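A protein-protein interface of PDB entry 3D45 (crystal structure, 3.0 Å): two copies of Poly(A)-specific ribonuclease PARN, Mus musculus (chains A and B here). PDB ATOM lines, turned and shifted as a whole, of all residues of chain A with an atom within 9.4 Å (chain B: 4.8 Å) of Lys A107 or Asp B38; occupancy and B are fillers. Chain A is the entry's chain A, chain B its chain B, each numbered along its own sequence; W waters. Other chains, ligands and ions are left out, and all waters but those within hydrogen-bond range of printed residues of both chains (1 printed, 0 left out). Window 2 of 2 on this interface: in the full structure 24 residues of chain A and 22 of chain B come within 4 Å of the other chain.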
ATOM      1  N   SER A  34     -14.059  25.630  25.472  1.00  0.00           N
ATOM      2  CA  SER A  34     -14.690  25.830  26.771  1.00  0.00           C
ATOM      3  C   SER A  34     -14.048  25.010  27.908  1.00  0.00           C
ATOM      4  O   SER A  34     -14.129  25.397  29.096  1.00  0.00           O
ATOM      5  CB  SER A  34     -16.126  25.383  26.625  1.00  0.00           C
ATOM      6  OG  SER A  34     -16.924  26.030  27.561  1.00  0.00           O
ATOM      7  N   MET A  64     -17.023  16.398  24.182  1.00  0.00           N
ATOM      8  CA  MET A  64     -17.748  17.131  23.155  1.00  0.00           C
ATOM      9  C   MET A  64     -18.890  18.067  23.648  1.00  0.00           C
ATOM     10  O   MET A  64     -19.513  18.791  22.843  1.00  0.00           O
ATOM     11  CB  MET A  64     -18.118  16.209  21.976  1.00  0.00           C
ATOM     12  CG  MET A  64     -17.569  16.710  20.604  1.00  0.00           C
ATOM     13  SD  MET A  64     -15.786  17.006  20.497  1.00  0.00           S
ATOM     14  CE  MET A  64     -15.201  15.464  21.152  1.00  0.00           C
ATOM     15  N   ASP A  65     -19.139  18.098  24.952  1.00  0.00           N
ATOM     16  CA  ASP A  65     -20.116  19.044  25.461  1.00  0.00           C
ATOM     17  C   ASP A  65     -19.487  20.414  25.619  1.00  0.00           C
ATOM     18  O   ASP A  65     -20.175  21.377  26.016  1.00  0.00           O
ATOM     19  CB  ASP A  65     -20.654  18.597  26.813  1.00  0.00           C
ATOM     20  CG  ASP A  65     -21.571  17.395  26.717  1.00  0.00           C
ATOM     21  OD1 ASP A  65     -22.023  17.032  25.593  1.00  0.00           O
ATOM     22  OD2 ASP A  65     -21.846  16.813  27.792  1.00  0.00           O
ATOM     23  N   PHE A  66     -18.180  20.487  25.349  1.00  0.00           N
ATOM     24  CA  PHE A  66     -17.441  21.761  25.466  1.00  0.00           C
ATOM     25  C   PHE A  66     -17.517  22.562  24.175  1.00  0.00           C
ATOM     26  O   PHE A  66     -17.578  21.988  23.096  1.00  0.00           O
ATOM     27  CB  PHE A  66     -15.981  21.533  25.864  1.00  0.00           C
ATOM     28  CG  PHE A  66     -15.819  20.966  27.237  1.00  0.00           C
ATOM     29  CD1 PHE A  66     -15.550  19.628  27.422  1.00  0.00           C
ATOM     30  CD2 PHE A  66     -15.954  21.774  28.362  1.00  0.00           C
ATOM     31  CE1 PHE A  66     -15.398  19.114  28.710  1.00  0.00           C
ATOM     32  CE2 PHE A  66     -15.797  21.261  29.657  1.00  0.00           C
ATOM     33  CZ  PHE A  66     -15.522  19.939  29.823  1.00  0.00           C
ATOM     34  N   LEU A  67     -17.502  23.879  24.299  1.00  0.00           N
ATOM     35  CA  LEU A  67     -17.663  24.758  23.161  1.00  0.00           C
ATOM     36  C   LEU A  67     -16.347  25.223  22.559  1.00  0.00           C
ATOM     37  O   LEU A  67     -15.476  25.790  23.249  1.00  0.00           O
ATOM     38  CB  LEU A  67     -18.446  25.978  23.588  1.00  0.00           C
ATOM     39  CG  LEU A  67     -19.315  26.585  22.509  1.00  0.00           C
ATOM     40  CD1 LEU A  67     -20.287  25.513  21.942  1.00  0.00           C
ATOM     41  CD2 LEU A  67     -20.049  27.812  23.122  1.00  0.00           C
ATOM     42  N   PHE A  95     -20.031  31.770  18.616  1.00  0.00           N
ATOM     43  CA  PHE A  95     -21.006  31.574  19.715  1.00  0.00           C
ATOM     44  C   PHE A  95     -22.430  31.255  19.206  1.00  0.00           C
ATOM     45  O   PHE A  95     -23.018  32.038  18.426  1.00  0.00           O
ATOM     46  CB  PHE A  95     -21.057  32.803  20.639  1.00  0.00           C
ATOM     47  CG  PHE A  95     -22.163  32.763  21.656  1.00  0.00           C
ATOM     48  CD1 PHE A  95     -22.052  31.974  22.799  1.00  0.00           C
ATOM     49  CD2 PHE A  95     -23.299  33.526  21.492  1.00  0.00           C
ATOM     50  CE1 PHE A  95     -23.071  31.923  23.768  1.00  0.00           C
ATOM     51  CE2 PHE A  95     -24.341  33.486  22.458  1.00  0.00           C
ATOM     52  CZ  PHE A  95     -24.213  32.674  23.594  1.00  0.00           C
ATOM     53  N   PRO A  96     -22.992  30.118  19.653  1.00  0.00           N
ATOM     54  CA  PRO A  96     -24.297  29.705  19.205  1.00  0.00           C
ATOM     55  C   PRO A  96     -25.433  30.565  19.758  1.00  0.00           C
ATOM     56  O   PRO A  96     -26.308  30.039  20.449  1.00  0.00           O
ATOM     57  CB  PRO A  96     -24.408  28.268  19.729  1.00  0.00           C
ATOM     58  CG  PRO A  96     -23.540  28.216  20.865  1.00  0.00           C
ATOM     59  CD  PRO A  96     -22.408  29.148  20.589  1.00  0.00           C
ATOM     60  N   PRO A  98     -28.850  31.787  19.785  1.00  0.00           N
ATOM     61  CA  PRO A  98     -30.060  31.295  19.106  1.00  0.00           C
ATOM     62  C   PRO A  98     -30.593  32.233  18.018  1.00  0.00           C
ATOM     63  O   PRO A  98     -30.494  33.458  18.130  1.00  0.00           O
ATOM     64  CB  PRO A  98     -31.078  31.115  20.239  1.00  0.00           C
ATOM     65  CG  PRO A  98     -30.462  31.732  21.445  1.00  0.00           C
ATOM     66  CD  PRO A  98     -28.999  31.782  21.254  1.00  0.00           C
ATOM     67  N   SER A 103     -35.757  28.109  17.344  1.00  0.00           N
ATOM     68  CA  SER A 103     -34.409  27.628  17.047  1.00  0.00           C
ATOM     69  C   SER A 103     -33.779  26.885  18.259  1.00  0.00           C
ATOM     70  O   SER A 103     -34.006  27.273  19.417  1.00  0.00           O
ATOM     71  CB  SER A 103     -33.574  28.847  16.681  1.00  0.00           C
ATOM     72  OG  SER A 103     -32.419  28.478  15.976  1.00  0.00           O
ATOM     73  N   PRO A 104     -33.004  25.806  18.027  1.00  0.00           N
ATOM     74  CA  PRO A 104     -32.455  25.134  19.231  1.00  0.00           C
ATOM     75  C   PRO A 104     -31.558  26.041  20.101  1.00  0.00           C
ATOM     76  O   PRO A 104     -30.783  26.834  19.560  1.00  0.00           O
ATOM     77  CB  PRO A 104     -31.650  23.959  18.652  1.00  0.00           C
ATOM     78  CG  PRO A 104     -32.213  23.735  17.290  1.00  0.00           C
ATOM     79  CD  PRO A 104     -32.600  25.116  16.790  1.00  0.00           C
ATOM     80  N   ASP A 105     -31.694  25.925  21.429  1.00  0.00           N
ATOM     81  CA  ASP A 105     -30.950  26.731  22.434  1.00  0.00           C
ATOM     82  C   ASP A 105     -29.783  25.932  23.014  1.00  0.00           C
ATOM     83  O   ASP A 105     -29.978  25.150  23.941  1.00  0.00           O
ATOM     84  CB  ASP A 105     -31.910  27.143  23.574  1.00  0.00           C
ATOM     85  CG  ASP A 105     -31.255  28.026  24.670  1.00  0.00           C
ATOM     86  OD1 ASP A 105     -31.912  28.189  25.712  1.00  0.00           O
ATOM     87  OD2 ASP A 105     -30.130  28.565  24.525  1.00  0.00           O
ATOM     88  N   VAL A 106     -28.570  26.136  22.493  1.00  0.00           N
ATOM     89  CA  VAL A 106     -27.435  25.275  22.863  1.00  0.00           C
ATOM     90  C   VAL A 106     -26.976  25.402  24.326  1.00  0.00           C
ATOM     91  O   VAL A 106     -26.875  26.507  24.865  1.00  0.00           O
ATOM     92  CB  VAL A 106     -26.257  25.391  21.878  1.00  0.00           C
ATOM     93  CG1 VAL A 106     -24.935  25.232  22.575  1.00  0.00           C
ATOM     94  CG2 VAL A 106     -26.382  24.327  20.873  1.00  0.00           C
ATOM     95  N   LYS A 107     -26.734  24.250  24.969  1.00  0.00           N
ATOM     96  CA  LYS A 107     -26.250  24.209  26.359  1.00  0.00           C
ATOM     97  C   LYS A 107     -24.872  23.632  26.310  1.00  0.00           C
ATOM     98  O   LYS A 107     -24.709  22.452  26.085  1.00  0.00           O
ATOM     99  CB  LYS A 107     -27.111  23.339  27.337  1.00  0.00           C
ATOM    100  CG  LYS A 107     -28.656  23.520  27.333  1.00  0.00           C
ATOM    101  CD  LYS A 107     -29.303  22.584  26.253  1.00  0.00           C
ATOM    102  CE  LYS A 107     -30.832  22.613  26.153  1.00  0.00           C
ATOM    103  NZ  LYS A 107     -31.290  23.983  25.914  1.00  0.00           N
ATOM    104  N   PHE A 108     -23.861  24.456  26.511  1.00  0.00           N
ATOM    105  CA  PHE A 108     -22.484  23.950  26.526  1.00  0.00           C
ATOM    106  C   PHE A 108     -21.922  23.875  27.921  1.00  0.00           C
ATOM    107  O   PHE A 108     -22.453  24.461  28.870  1.00  0.00           O
ATOM    108  CB  PHE A 108     -21.550  24.803  25.680  1.00  0.00           C
ATOM    109  CG  PHE A 108     -21.506  26.227  26.072  1.00  0.00           C
ATOM    110  CD1 PHE A 108     -20.495  26.701  26.888  1.00  0.00           C
ATOM    111  CD2 PHE A 108     -22.450  27.117  25.599  1.00  0.00           C
ATOM    112  CE1 PHE A 108     -20.451  28.063  27.252  1.00  0.00           C
ATOM    113  CE2 PHE A 108     -22.413  28.464  25.949  1.00  0.00           C
ATOM    114  CZ  PHE A 108     -21.420  28.940  26.778  1.00  0.00           C
ATOM    115  N   VAL A 109     -20.818  23.173  28.059  1.00  0.00           N
ATOM    116  CA  VAL A 109     -20.194  23.037  29.365  1.00  0.00           C
ATOM    117  C   VAL A 109     -18.915  23.844  29.440  1.00  0.00           C
ATOM    118  O   VAL A 109     -18.200  23.942  28.455  1.00  0.00           O
ATOM    119  CB  VAL A 109     -19.823  21.579  29.636  1.00  0.00           C
ATOM    120  CG1 VAL A 109     -19.193  21.422  31.002  1.00  0.00           C
ATOM    121  CG2 VAL A 109     -21.049  20.725  29.556  1.00  0.00           C
ATOM    122  N   CYS A 110     -18.627  24.402  30.614  1.00  0.00           N
ATOM    123  CA  CYS A 110     -17.327  25.013  30.904  1.00  0.00           C
ATOM    124  C   CYS A 110     -16.521  24.310  31.994  1.00  0.00           C
ATOM    125  O   CYS A 110     -17.033  24.018  33.063  1.00  0.00           O
ATOM    126  CB  CYS A 110     -17.477  26.428  31.417  1.00  0.00           C
ATOM    127  SG  CYS A 110     -18.227  27.538  30.343  1.00  0.00           S
ATOM    128  N   TYR A 135     -23.750  30.178  13.951  1.00  0.00           N
ATOM    129  CA  TYR A 135     -23.444  29.081  13.060  1.00  0.00           C
ATOM    130  C   TYR A 135     -24.545  28.036  13.123  1.00  0.00           C
ATOM    131  O   TYR A 135     -25.338  28.003  14.078  1.00  0.00           O
ATOM    132  CB  TYR A 135     -22.122  28.435  13.438  1.00  0.00           C
ATOM    133  CG  TYR A 135     -22.088  27.743  14.794  1.00  0.00           C
ATOM    134  CD1 TYR A 135     -22.223  26.345  14.895  1.00  0.00           C
ATOM    135  CD2 TYR A 135     -21.885  28.469  15.980  1.00  0.00           C
ATOM    136  CE1 TYR A 135     -22.170  25.696  16.135  1.00  0.00           C
ATOM    137  CE2 TYR A 135     -21.858  27.825  17.234  1.00  0.00           C
ATOM    138  CZ  TYR A 135     -21.990  26.439  17.301  1.00  0.00           C
ATOM    139  OH  TYR A 135     -21.946  25.781  18.526  1.00  0.00           O
ATOM    140  N   HIS A 293     -18.450  18.107  15.200  1.00  0.00           N
ATOM    141  CA  HIS A 293     -19.548  18.114  16.189  1.00  0.00           C
ATOM    142  C   HIS A 293     -20.371  19.401  16.126  1.00  0.00           C
ATOM    143  O   HIS A 293     -21.587  19.381  15.966  1.00  0.00           O
ATOM    144  CB  HIS A 293     -18.990  17.952  17.604  1.00  0.00           C
ATOM    145  CG  HIS A 293     -20.002  17.480  18.605  1.00  0.00           C
ATOM    146  ND1 HIS A 293     -20.422  18.258  19.668  1.00  0.00           N
ATOM    147  CD2 HIS A 293     -20.671  16.303  18.712  1.00  0.00           C
ATOM    148  CE1 HIS A 293     -21.309  17.585  20.380  1.00  0.00           C
ATOM    149  NE2 HIS A 293     -21.474  16.395  19.827  1.00  0.00           N
ATOM    150  N   GLN A 294     -19.675  20.522  16.245  1.00  0.00           N
ATOM    151  CA  GLN A 294     -20.303  21.827  16.217  1.00  0.00           C
ATOM    152  C   GLN A 294     -20.809  22.290  14.844  1.00  0.00           C
ATOM    153  O   GLN A 294     -21.852  22.959  14.786  1.00  0.00           O
ATOM    154  CB  GLN A 294     -19.364  22.860  16.848  1.00  0.00           C
ATOM    155  CG  GLN A 294     -19.480  22.790  18.355  1.00  0.00           C
ATOM    156  CD  GLN A 294     -18.324  23.390  19.115  1.00  0.00           C
ATOM    157  OE1 GLN A 294     -18.023  24.584  18.970  1.00  0.00           O
ATOM    158  NE2 GLN A 294     -17.687  22.572  19.969  1.00  0.00           N
ATOM    159  N   ILE B  36     -31.005  28.716  32.974  1.00  0.00           N
ATOM    160  CA  ILE B  36     -32.189  28.237  33.703  1.00  0.00           C
ATOM    161  C   ILE B  36     -32.399  26.720  33.569  1.00  0.00           C
ATOM    162  O   ILE B  36     -32.483  26.012  34.579  1.00  0.00           O
ATOM    163  CB  ILE B  36     -33.505  28.909  33.255  1.00  0.00           C
ATOM    164  CG1 ILE B  36     -33.452  30.420  33.426  1.00  0.00           C
ATOM    165  CG2 ILE B  36     -34.682  28.340  34.053  1.00  0.00           C
ATOM    166  CD1 ILE B  36     -33.815  30.914  34.849  1.00  0.00           C
ATOM    167  N   SER B  37     -32.505  26.224  32.334  1.00  0.00           N
ATOM    168  CA  SER B  37     -32.813  24.805  32.103  1.00  0.00           C
ATOM    169  C   SER B  37     -31.817  24.148  31.168  1.00  0.00           C
ATOM    170  O   SER B  37     -31.421  24.762  30.190  1.00  0.00           O
ATOM    171  CB  SER B  37     -34.226  24.664  31.503  1.00  0.00           C
ATOM    172  OG  SER B  37     -34.492  23.325  31.088  1.00  0.00           O
ATOM    173  N   ASP B  38     -31.427  22.905  31.454  1.00  0.00           N
ATOM    174  CA  ASP B  38     -30.746  22.077  30.449  1.00  0.00           C
ATOM    175  C   ASP B  38     -31.846  21.548  29.547  1.00  0.00           C
ATOM    176  O   ASP B  38     -32.582  22.360  28.976  1.00  0.00           O
ATOM    177  CB  ASP B  38     -29.900  20.980  31.080  1.00  0.00           C
ATOM    178  CG  ASP B  38     -30.679  20.104  32.025  1.00  0.00           C
ATOM    179  OD1 ASP B  38     -31.897  20.295  32.215  1.00  0.00           O
ATOM    180  OD2 ASP B  38     -30.066  19.189  32.589  1.00  0.00           O
ATOM    181  N   GLY B  39     -32.015  20.233  29.433  1.00  0.00           N
ATOM    182  CA  GLY B  39     -33.241  19.655  28.795  1.00  0.00           C
ATOM    183  C   GLY B  39     -34.571  20.447  28.666  1.00  0.00           C
ATOM    184  O   GLY B  39     -34.791  21.140  27.676  1.00  0.00           O
ATOM    185  N   PRO B  40     -35.473  20.348  29.664  1.00  0.00           N
ATOM    186  CA  PRO B  40     -36.874  20.759  29.556  1.00  0.00           C
ATOM    187  C   PRO B  40     -37.075  22.226  29.256  1.00  0.00           C
ATOM    188  O   PRO B  40     -36.205  23.018  29.539  1.00  0.00           O
ATOM    189  CB  PRO B  40     -37.405  20.494  30.956  1.00  0.00           C
ATOM    190  CG  PRO B  40     -36.542  19.474  31.493  1.00  0.00           C
ATOM    191  CD  PRO B  40     -35.189  19.823  31.007  1.00  0.00           C
ATOM    192  N   LYS B  61     -32.896  18.504  39.191  1.00  0.00           N
ATOM    193  CA  LYS B  61     -32.397  17.713  38.081  1.00  0.00           C
ATOM    194  C   LYS B  61     -32.019  18.548  36.868  1.00  0.00           C
ATOM    195  O   LYS B  61     -31.374  18.035  35.958  1.00  0.00           O
ATOM    196  CB  LYS B  61     -33.500  16.743  37.654  1.00  0.00           C
ATOM    197  CG  LYS B  61     -33.039  15.332  37.262  1.00  0.00           C
ATOM    198  CD  LYS B  61     -34.251  14.488  36.871  1.00  0.00           C
ATOM    199  CE  LYS B  61     -34.710  14.837  35.442  1.00  0.00           C
ATOM    200  NZ  LYS B  61     -36.203  14.781  35.208  1.00  0.00           N
ATOM    201  N   HIS B  62     -32.424  19.816  36.838  1.00  0.00           N
ATOM    202  CA  HIS B  62     -32.421  20.568  35.588  1.00  0.00           C
ATOM    203  C   HIS B  62     -31.885  21.995  35.662  1.00  0.00           C
ATOM    204  O   HIS B  62     -31.798  22.665  34.624  1.00  0.00           O
ATOM    205  CB  HIS B  62     -33.842  20.594  35.005  1.00  0.00           C
ATOM    206  CG  HIS B  62     -34.283  19.288  34.417  1.00  0.00           C
ATOM    207  ND1 HIS B  62     -35.553  18.776  34.610  1.00  0.00           N
ATOM    208  CD2 HIS B  62     -33.621  18.381  33.652  1.00  0.00           C
ATOM    209  CE1 HIS B  62     -35.651  17.614  33.985  1.00  0.00           C
ATOM    210  NE2 HIS B  62     -34.493  17.348  33.401  1.00  0.00           N
ATOM    211  N   PHE B  66     -26.012  25.068  36.681  1.00  0.00           N
ATOM    212  CA  PHE B  66     -25.746  26.420  36.219  1.00  0.00           C
ATOM    213  C   PHE B  66     -25.010  27.188  37.284  1.00  0.00           C
ATOM    214  O   PHE B  66     -25.125  26.892  38.484  1.00  0.00           O
ATOM    215  CB  PHE B  66     -27.006  27.102  35.701  1.00  0.00           C
ATOM    216  CG  PHE B  66     -27.572  26.401  34.522  1.00  0.00           C
ATOM    217  CD1 PHE B  66     -28.733  25.638  34.638  1.00  0.00           C
ATOM    218  CD2 PHE B  66     -26.883  26.425  33.290  1.00  0.00           C
ATOM    219  CE1 PHE B  66     -29.229  24.946  33.535  1.00  0.00           C
ATOM    220  CE2 PHE B  66     -27.369  25.734  32.169  1.00  0.00           C
ATOM    221  CZ  PHE B  66     -28.541  24.985  32.290  1.00  0.00           C
ATOM    222  N   VAL B 109     -22.514  24.743  33.630  1.00  0.00           N
ATOM    223  CA  VAL B 109     -23.109  24.731  32.307  1.00  0.00           C
ATOM    224  C   VAL B 109     -23.603  26.123  32.009  1.00  0.00           C
ATOM    225  O   VAL B 109     -23.956  26.845  32.932  1.00  0.00           O
ATOM    226  CB  VAL B 109     -24.225  23.645  32.180  1.00  0.00           C
ATOM    227  CG1 VAL B 109     -24.709  23.532  30.746  1.00  0.00           C
ATOM    228  CG2 VAL B 109     -23.716  22.317  32.610  1.00  0.00           C
ATOM    229  N   CYS B 110     -23.606  26.481  30.720  1.00  0.00           N
ATOM    230  CA  CYS B 110     -24.223  27.711  30.228  1.00  0.00           C
ATOM    231  C   CYS B 110     -25.385  27.473  29.280  1.00  0.00           C
ATOM    232  O   CYS B 110     -25.352  26.536  28.486  1.00  0.00           O
ATOM    233  CB  CYS B 110     -23.175  28.531  29.502  1.00  0.00           C
ATOM    234  SG  CYS B 110     -21.942  29.070  30.621  1.00  0.00           S
ATOM    235  N   GLN B 111     -26.384  28.349  29.339  1.00  0.00           N
ATOM    236  CA  GLN B 111     -27.511  28.296  28.452  1.00  0.00           C
ATOM    237  C   GLN B 111     -27.513  29.557  27.619  1.00  0.00           C
ATOM    238  O   GLN B 111     -27.583  30.688  28.153  1.00  0.00           O
ATOM    239  CB  GLN B 111     -28.753  28.159  29.282  1.00  0.00           C
ATOM    240  CG  GLN B 111     -29.982  28.502  28.566  1.00  0.00           C
ATOM    241  CD  GLN B 111     -31.157  27.935  29.254  1.00  0.00           C
ATOM    242  OE1 GLN B 111     -32.094  27.485  28.614  1.00  0.00           O
ATOM    243  NE2 GLN B 111     -31.110  27.903  30.576  1.00  0.00           N
ATOM    244  N   SER B 112     -27.467  29.337  26.304  1.00  0.00           N
ATOM    245  CA  SER B 112     -27.148  30.350  25.311  1.00  0.00           C
ATOM    246  C   SER B 112     -28.074  31.534  25.347  1.00  0.00           C
ATOM    247  O   SER B 112     -27.620  32.668  25.237  1.00  0.00           O
ATOM    248  CB  SER B 112     -27.097  29.721  23.938  1.00  0.00           C
ATOM    249  OG  SER B 112     -26.173  28.652  23.944  1.00  0.00           O
HETATM  250  O   HOH W   1     -34.177  22.805  25.304  1.00  0.00           O
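Of the 19 printed residues of chain A, 7 touch a printed residue of chain B. Printed residues of chain A that touch a printed residue of chain B: Phe A95, Pro A96, Pro A98, Asp A105, Val A106, Lys A107 and Phe A108. Hydrophobic or aromatic side chains of chain A within 4 Å of the printed part of chain B: Phe A95, Pro A98, Val A106 and Phe A108. Of the 12 printed residues of chain B, 5 touch a printed residue of chain A. Printed residues of chain B that touch a printed residue of chain A: Asp B38, Val B109, Cys B110, Gln B111 and Ser B112. Along chain B the printed residues that touch a printed residue of chain A span positions 38 to 112. Among the printed residues, no Asp or Glu carboxylate lies within 4 Å of a Lys or Arg side-chain nitrogen of the other chain.
Water W1 bridges the backbone carbonyl oxygen (O) of Gly B39 and the side-chain amino group (NZ) of Lys A107.
The backbone carbonyl oxygen (O) of Asp A105 sits at hydrogen-bond distance from the side-chain amino group (NZ) of Lys A107. N of Ile B36 lies close to NE2 of Gln B111 (2.5 Å). The backbone NH (N) of Ser B37 sits close to the side-chain amide nitrogen (NE2) of Gln B111 (2.8 Å). The backbone NH (N) of Asp B38 is in hydrogen-bond range of the backbone carbonyl oxygen (O) of His B62 (3.2 Å).
The side-chain carboxylate (OD1) of Asp A105 lies close to the side-chain amide oxygen (OE1) of Gln B111 (3.0 Å). The backbone NH (N) of Ser B112 lies within hydrogen-bond range of the side-chain carboxylate (OD2) of Asp A105 (3.3 Å). OG of Ser B112 sits at hydrogen-bond distance from O of Val A106, at 2.4 Å. N of Cys B110 sits at hydrogen-bond distance from O of Phe A108 (3.0 Å).
Phe A95 touches Ser B112 (CZ to O, 3.8 Å). Ser B112 touches Pro A96. Ser B112 touches Pro A98 (CB to CD, 3.9 Å). Cys B110 touches Val A106. CE of Lys A107 touches O of Asp B38 (3.3 Å). CA of Lys A107 touches O of Cys B110, at 3.3 Å. Val B109 touches Phe A108 (CG1 to O, 3.1 Å).
Positions printed for both chains: 66, 109 and 110.
Of the printed residues of chain B, Pro A96 touches Ser B112 (3.6 Å). Lys A107 touches just these residues of chain B: Asp B38 and Cys B110. Printed residues of chain B within 4 Å of Phe A108: Val B109 and Cys B110. No residue of chain A comes within 4 Å of Ser B37. Asp B38 touches one residue of chain A. No residue of chain A comes within 4 Å of Gly B39. Lys B61 touches none of the printed residues of chain A. Phe B66 touches none of the printed residues of chain A. Of the printed residues of chain A, Ser B112 touches Phe A95 (3.8 Å), Pro A96 (3.6 Å), Pro A98 (3.9 Å), Asp A105 (3.3 Å) and Val A106 (2.4 Å). The nearest printed residue of chain B that does not touch Lys A107 is Ser B37 (4.2 Å). The nearest residue of chain A that does not touch Asp B38 is Asp A105 (6.3 Å).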
